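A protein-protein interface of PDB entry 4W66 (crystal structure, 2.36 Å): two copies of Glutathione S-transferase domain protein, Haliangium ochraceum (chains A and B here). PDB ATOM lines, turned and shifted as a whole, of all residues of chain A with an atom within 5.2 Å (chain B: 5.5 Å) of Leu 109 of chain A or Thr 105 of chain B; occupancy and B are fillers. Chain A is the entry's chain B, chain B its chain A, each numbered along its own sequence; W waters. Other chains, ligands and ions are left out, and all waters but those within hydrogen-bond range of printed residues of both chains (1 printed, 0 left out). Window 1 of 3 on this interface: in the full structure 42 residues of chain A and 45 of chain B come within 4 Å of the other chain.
Water W1 bridges the side-chain hydroxyl (OH) of Tyr 104 of chain B and the side-chain hydroxyl (OG1) of Thr 105 of chain A.
The side-chain carboxylate (OE2) of Glu 106 of chain B is in salt-bridge range of the guanidinium group (NH1) of Arg 18 of chain A, at 3.7 Å.
Leu 109 of chain A touches Thr 105 of chain B, but with the chains exchanged Thr 105 of chain A does not touch Leu 109 of chain B (4.7 Å). Positions printed for both chains: 103, 104, 105, 107, 108, 109 and 110.
Hydrophobic or aromatic side chains of chain A that line the printed part of chain B: Leu 109. Among the printed residues, Asp or Glu carboxylates within 4 Å of a Lys or Arg side-chain nitrogen of the other chain: Arg 18 of chain A with Glu 106 of chain B.
O of Ser 101 of chain B sits close to OG1 of Thr 105 of chain B, 3.2 Å away. The backbone carbonyl oxygen (O) of Tyr 104 of chain A sits at hydrogen-bond distance from the backbone NH (N) of Leu 109 of chain A, at 2.8 Å.
Of the printed residues of chain B, Arg 18 of chain A touches Glu 106. Printed residues of chain B within 4 Å of Leu 109 of chain A: Thr 105. Of the printed residues of chain A, Thr 105 of chain B touches Leu 109 (3.95 Å). Of the printed residues of chain A, Glu 106 of chain B touches Arg 18. The nearest printed residue of chain B that does not touch Leu 109 of chain A is Glu 106 of chain B (5.7 Å). The nearest printed residue of chain B that does not touch Arg 18 of chain A is Thr 105 of chain B (5.9 Å).
Among the printed residues, merely in contact across the chains: Leu 109 of chain A with Thr 105 of chain B.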
ATOM      1  N   ARG A  18      21.658  27.718  11.245  1.00  0.00           N
ATOM      2  CA  ARG A  18      21.289  26.666  12.193  1.00  0.00           C
ATOM      3  C   ARG A  18      20.231  27.087  13.175  1.00  0.00           C
ATOM      4  O   ARG A  18      19.863  26.285  14.021  1.00  0.00           O
ATOM      5  CB  ARG A  18      22.519  26.218  13.006  1.00  0.00           C
ATOM      6  CG  ARG A  18      23.686  25.797  12.140  1.00  0.00           C
ATOM      7  CD  ARG A  18      24.861  25.244  12.933  1.00  0.00           C
ATOM      8  NE  ARG A  18      25.819  24.643  12.001  1.00  0.00           N
ATOM      9  CZ  ARG A  18      26.845  23.863  12.334  1.00  0.00           C
ATOM     10  NH1 ARG A  18      27.101  23.569  13.596  1.00  0.00           N
ATOM     11  NH2 ARG A  18      27.621  23.368  11.389  1.00  0.00           N
ATOM     12  N   CYS A 103      15.378  17.536   7.599  1.00  0.00           N
ATOM     13  CA  CYS A 103      15.406  18.928   7.184  1.00  0.00           C
ATOM     14  C   CYS A 103      16.699  19.635   7.572  1.00  0.00           C
ATOM     15  O   CYS A 103      17.283  20.336   6.756  1.00  0.00           O
ATOM     16  CB  CYS A 103      14.187  19.674   7.724  1.00  0.00           C
ATOM     17  SG  CYS A 103      12.695  19.178   6.848  1.00  0.00           S
ATOM     18  N   TYR A 104      17.162  19.429   8.795  1.00  0.00           N
ATOM     19  CA  TYR A 104      18.378  20.075   9.254  1.00  0.00           C
ATOM     20  C   TYR A 104      19.631  19.417   8.678  1.00  0.00           C
ATOM     21  O   TYR A 104      20.458  20.088   8.063  1.00  0.00           O
ATOM     22  CB  TYR A 104      18.424  20.068  10.778  1.00  0.00           C
ATOM     23  CG  TYR A 104      19.673  20.640  11.400  1.00  0.00           C
ATOM     24  CD1 TYR A 104      19.917  22.021  11.409  1.00  0.00           C
ATOM     25  CD2 TYR A 104      20.596  19.810  12.013  1.00  0.00           C
ATOM     26  CE1 TYR A 104      21.060  22.547  12.016  1.00  0.00           C
ATOM     27  CE2 TYR A 104      21.728  20.318  12.618  1.00  0.00           C
ATOM     28  CZ  TYR A 104      21.964  21.686  12.619  1.00  0.00           C
ATOM     29  OH  TYR A 104      23.126  22.164  13.219  1.00  0.00           O
ATOM     30  N   THR A 105      19.799  18.120   8.867  1.00  0.00           N
ATOM     31  CA  THR A 105      21.077  17.527   8.498  1.00  0.00           C
ATOM     32  C   THR A 105      21.236  17.298   7.014  1.00  0.00           C
ATOM     33  O   THR A 105      22.345  17.347   6.522  1.00  0.00           O
ATOM     34  CB  THR A 105      21.393  16.210   9.244  1.00  0.00           C
ATOM     35  OG1 THR A 105      20.509  15.175   8.811  1.00  0.00           O
ATOM     36  CG2 THR A 105      21.283  16.400  10.742  1.00  0.00           C
ATOM     37  N   VAL A 107      19.458  18.952   4.506  1.00  0.00           N
ATOM     38  CA  VAL A 107      19.073  20.066   3.653  1.00  0.00           C
ATOM     39  C   VAL A 107      19.713  21.362   4.120  1.00  0.00           C
ATOM     40  O   VAL A 107      20.625  21.857   3.462  1.00  0.00           O
ATOM     41  CB  VAL A 107      17.553  20.199   3.540  1.00  0.00           C
ATOM     42  CG1 VAL A 107      17.178  21.395   2.675  1.00  0.00           C
ATOM     43  CG2 VAL A 107      16.959  18.928   2.961  1.00  0.00           C
ATOM     44  N   SER A 108      19.267  21.908   5.242  1.00  0.00           N
ATOM     45  CA  SER A 108      19.863  23.140   5.763  1.00  0.00           C
ATOM     46  C   SER A 108      21.384  23.076   5.959  1.00  0.00           C
ATOM     47  O   SER A 108      22.087  23.985   5.533  1.00  0.00           O
ATOM     48  CB  SER A 108      19.209  23.551   7.076  1.00  0.00           C
ATOM     49  OG  SER A 108      17.856  23.889   6.847  1.00  0.00           O
ATOM     50  N   LEU A 109      21.896  22.029   6.605  1.00  0.00           N
ATOM     51  CA  LEU A 109      23.349  21.913   6.763  1.00  0.00           C
ATOM     52  C   LEU A 109      24.076  21.808   5.422  1.00  0.00           C
ATOM     53  O   LEU A 109      25.191  22.285   5.305  1.00  0.00           O
ATOM     54  CB  LEU A 109      23.752  20.718   7.620  1.00  0.00           C
ATOM     55  CG  LEU A 109      23.749  20.894   9.138  1.00  0.00           C
ATOM     56  CD1 LEU A 109      24.440  19.689   9.743  1.00  0.00           C
ATOM     57  CD2 LEU A 109      24.446  22.166   9.599  1.00  0.00           C
ATOM     58  N   GLN A 110      23.454  21.178   4.427  1.00  0.00           N
ATOM     59  CA  GLN A 110      24.106  20.975   3.130  1.00  0.00           C
ATOM     60  C   GLN A 110      24.104  22.262   2.301  1.00  0.00           C
ATOM     61  O   GLN A 110      25.049  22.526   1.566  1.00  0.00           O
ATOM     62  CB  GLN A 110      23.463  19.829   2.345  1.00  0.00           C
ATOM     63  CG  GLN A 110      23.406  18.512   3.110  1.00  0.00           C
ATOM     64  CD  GLN A 110      24.766  18.034   3.617  1.00  0.00           C
ATOM     65  OE1 GLN A 110      25.740  17.976   2.865  1.00  0.00           O
ATOM     66  NE2 GLN A 110      24.829  17.663   4.895  1.00  0.00           N
ATOM     67  N   ILE A 111      23.063  23.071   2.457  1.00  0.00           N
ATOM     68  CA  ILE A 111      23.007  24.371   1.815  1.00  0.00           C
ATOM     69  C   ILE A 111      24.138  25.219   2.350  1.00  0.00           C
ATOM     70  O   ILE A 111      24.858  25.851   1.582  1.00  0.00           O
ATOM     71  CB  ILE A 111      21.674  25.087   2.078  1.00  0.00           C
ATOM     72  CG1 ILE A 111      20.512  24.344   1.406  1.00  0.00           C
ATOM     73  CG2 ILE A 111      21.737  26.545   1.641  1.00  0.00           C
ATOM     74  CD1 ILE A 111      20.433  24.533  -0.083  1.00  0.00           C
ATOM     75  N   ALA A 112      24.304  25.230   3.665  1.00  0.00           N
ATOM     76  CA  ALA A 112      25.451  25.909   4.266  1.00  0.00           C
ATOM     77  C   ALA A 112      26.769  25.385   3.687  1.00  0.00           C
ATOM     78  O   ALA A 112      27.665  26.152   3.369  1.00  0.00           O
ATOM     79  CB  ALA A 112      25.440  25.748   5.772  1.00  0.00           C
ATOM     80  N   GLN A 113      26.883  24.071   3.558  1.00  0.00           N
ATOM     81  CA  GLN A 113      28.111  23.477   3.037  1.00  0.00           C
ATOM     82  C   GLN A 113      28.452  23.969   1.643  1.00  0.00           C
ATOM     83  O   GLN A 113      29.618  24.206   1.337  1.00  0.00           O
ATOM     84  CB  GLN A 113      28.028  21.954   3.038  1.00  0.00           C
ATOM     85  CG  GLN A 113      28.925  21.319   4.067  1.00  0.00           C
ATOM     86  CD  GLN A 113      28.475  19.926   4.409  1.00  0.00           C
ATOM     87  OE1 GLN A 113      28.618  18.988   3.607  1.00  0.00           O
ATOM     88  NE2 GLN A 113      27.923  19.772   5.606  1.00  0.00           N
ATOM     89  N   VAL B 100      24.866  12.775  21.565  1.00  0.00           N
ATOM     90  CA  VAL B 100      24.529  11.986  20.391  1.00  0.00           C
ATOM     91  C   VAL B 100      24.627  12.873  19.152  1.00  0.00           C
ATOM     92  O   VAL B 100      25.252  12.510  18.160  1.00  0.00           O
ATOM     93  CB  VAL B 100      23.091  11.429  20.470  1.00  0.00           C
ATOM     94  CG1 VAL B 100      22.635  10.854  19.128  1.00  0.00           C
ATOM     95  CG2 VAL B 100      22.984  10.355  21.540  1.00  0.00           C
ATOM     96  N   SER B 101      23.991  14.032  19.220  1.00  0.00           N
ATOM     97  CA  SER B 101      23.885  14.890  18.056  1.00  0.00           C
ATOM     98  C   SER B 101      25.263  15.330  17.570  1.00  0.00           C
ATOM     99  O   SER B 101      25.529  15.348  16.369  1.00  0.00           O
ATOM    100  CB  SER B 101      23.035  16.109  18.359  1.00  0.00           C
ATOM    101  OG  SER B 101      23.372  17.136  17.441  1.00  0.00           O
ATOM    102  N   LEU B 102      26.130  15.669  18.515  1.00  0.00           N
ATOM    103  CA  LEU B 102      27.501  16.088  18.221  1.00  0.00           C
ATOM    104  C   LEU B 102      28.328  14.953  17.611  1.00  0.00           C
ATOM    105  O   LEU B 102      29.014  15.149  16.624  1.00  0.00           O
ATOM    106  CB  LEU B 102      28.155  16.565  19.507  1.00  0.00           C
ATOM    107  CG  LEU B 102      29.572  17.120  19.426  1.00  0.00           C
ATOM    108  CD1 LEU B 102      29.822  18.032  20.609  1.00  0.00           C
ATOM    109  CD2 LEU B 102      30.625  16.020  19.382  1.00  0.00           C
ATOM    110  N   CYS B 103      28.248  13.765  18.200  1.00  0.00           N
ATOM    111  CA  CYS B 103      28.960  12.609  17.682  1.00  0.00           C
ATOM    112  C   CYS B 103      28.492  12.224  16.305  1.00  0.00           C
ATOM    113  O   CYS B 103      29.292  11.834  15.463  1.00  0.00           O
ATOM    114  CB  CYS B 103      28.811  11.407  18.631  1.00  0.00           C
ATOM    115  SG  CYS B 103      29.617  11.738  20.218  1.00  0.00           S
ATOM    116  N   TYR B 104      27.200  12.337  16.053  1.00  0.00           N
ATOM    117  CA  TYR B 104      26.698  11.938  14.761  1.00  0.00           C
ATOM    118  C   TYR B 104      26.992  13.000  13.706  1.00  0.00           C
ATOM    119  O   TYR B 104      27.497  12.703  12.639  1.00  0.00           O
ATOM    120  CB  TYR B 104      25.219  11.649  14.851  1.00  0.00           C
ATOM    121  CG  TYR B 104      24.546  11.386  13.533  1.00  0.00           C
ATOM    122  CD1 TYR B 104      24.720  10.178  12.863  1.00  0.00           C
ATOM    123  CD2 TYR B 104      23.737  12.335  12.961  1.00  0.00           C
ATOM    124  CE1 TYR B 104      24.084   9.932  11.656  1.00  0.00           C
ATOM    125  CE2 TYR B 104      23.100  12.104  11.755  1.00  0.00           C
ATOM    126  CZ  TYR B 104      23.271  10.900  11.108  1.00  0.00           C
ATOM    127  OH  TYR B 104      22.628  10.701   9.896  1.00  0.00           O
ATOM    128  N   THR B 105      26.661  14.237  14.006  1.00  0.00           N
ATOM    129  CA  THR B 105      26.768  15.299  13.017  1.00  0.00           C
ATOM    130  C   THR B 105      28.214  15.681  12.752  1.00  0.00           C
ATOM    131  O   THR B 105      28.635  15.760  11.608  1.00  0.00           O
ATOM    132  CB  THR B 105      26.014  16.552  13.492  1.00  0.00           C
ATOM    133  OG1 THR B 105      24.613  16.296  13.425  1.00  0.00           O
ATOM    134  CG2 THR B 105      26.313  17.720  12.610  1.00  0.00           C
ATOM    135  N   GLU B 106      28.968  15.911  13.818  1.00  0.00           N
ATOM    136  CA  GLU B 106      30.281  16.509  13.705  1.00  0.00           C
ATOM    137  C   GLU B 106      31.377  15.481  13.536  1.00  0.00           C
ATOM    138  O   GLU B 106      32.482  15.840  13.175  1.00  0.00           O
ATOM    139  CB  GLU B 106      30.577  17.392  14.918  1.00  0.00           C
ATOM    140  CG  GLU B 106      29.503  18.437  15.221  1.00  0.00           C
ATOM    141  CD  GLU B 106      29.448  19.587  14.213  1.00  0.00           C
ATOM    142  OE1 GLU B 106      30.525  20.054  13.756  1.00  0.00           O
ATOM    143  OE2 GLU B 106      28.321  20.060  13.896  1.00  0.00           O
ATOM    144  N   VAL B 107      31.091  14.207  13.775  1.00  0.00           N
ATOM    145  CA  VAL B 107      32.134  13.178  13.693  1.00  0.00           C
ATOM    146  C   VAL B 107      31.790  12.107  12.688  1.00  0.00           C
ATOM    147  O   VAL B 107      32.493  11.926  11.713  1.00  0.00           O
ATOM    148  CB  VAL B 107      32.401  12.534  15.068  1.00  0.00           C
ATOM    149  CG1 VAL B 107      33.413  11.398  14.963  1.00  0.00           C
ATOM    150  CG2 VAL B 107      32.891  13.598  16.032  1.00  0.00           C
ATOM    151  N   SER B 108      30.710  11.392  12.914  1.00  0.00           N
ATOM    152  CA  SER B 108      30.389  10.287  12.034  1.00  0.00           C
ATOM    153  C   SER B 108      30.068  10.715  10.605  1.00  0.00           C
ATOM    154  O   SER B 108      30.541  10.075   9.665  1.00  0.00           O
ATOM    155  CB  SER B 108      29.289   9.433  12.639  1.00  0.00           C
ATOM    156  OG  SER B 108      29.829   8.797  13.798  1.00  0.00           O
ATOM    157  N   LEU B 109      29.289  11.779  10.424  1.00  0.00           N
ATOM    158  CA  LEU B 109      29.021  12.256   9.073  1.00  0.00           C
ATOM    159  C   LEU B 109      30.274  12.881   8.450  1.00  0.00           C
ATOM    160  O   LEU B 109      30.460  12.780   7.245  1.00  0.00           O
ATOM    161  CB  LEU B 109      27.875  13.275   9.016  1.00  0.00           C
ATOM    162  CG  LEU B 109      26.424  12.867   9.326  1.00  0.00           C
ATOM    163  CD1 LEU B 109      25.461  13.936   8.832  1.00  0.00           C
ATOM    164  CD2 LEU B 109      26.043  11.521   8.722  1.00  0.00           C
ATOM    165  N   GLN B 110      31.113  13.536   9.260  1.00  0.00           N
ATOM    166  CA  GLN B 110      32.291  14.213   8.736  1.00  0.00           C
ATOM    167  C   GLN B 110      33.397  13.234   8.357  1.00  0.00           C
ATOM    168  O   GLN B 110      34.060  13.425   7.353  1.00  0.00           O
ATOM    169  CB  GLN B 110      32.810  15.274   9.714  1.00  0.00           C
ATOM    170  CG  GLN B 110      31.882  16.475   9.883  1.00  0.00           C
ATOM    171  CD  GLN B 110      31.690  17.310   8.603  1.00  0.00           C
ATOM    172  OE1 GLN B 110      32.396  17.145   7.608  1.00  0.00           O
ATOM    173  NE2 GLN B 110      30.729  18.217   8.637  1.00  0.00           N
HETATM  174  O   HOH W   1      21.366  12.535   8.553  1.00  0.00           O
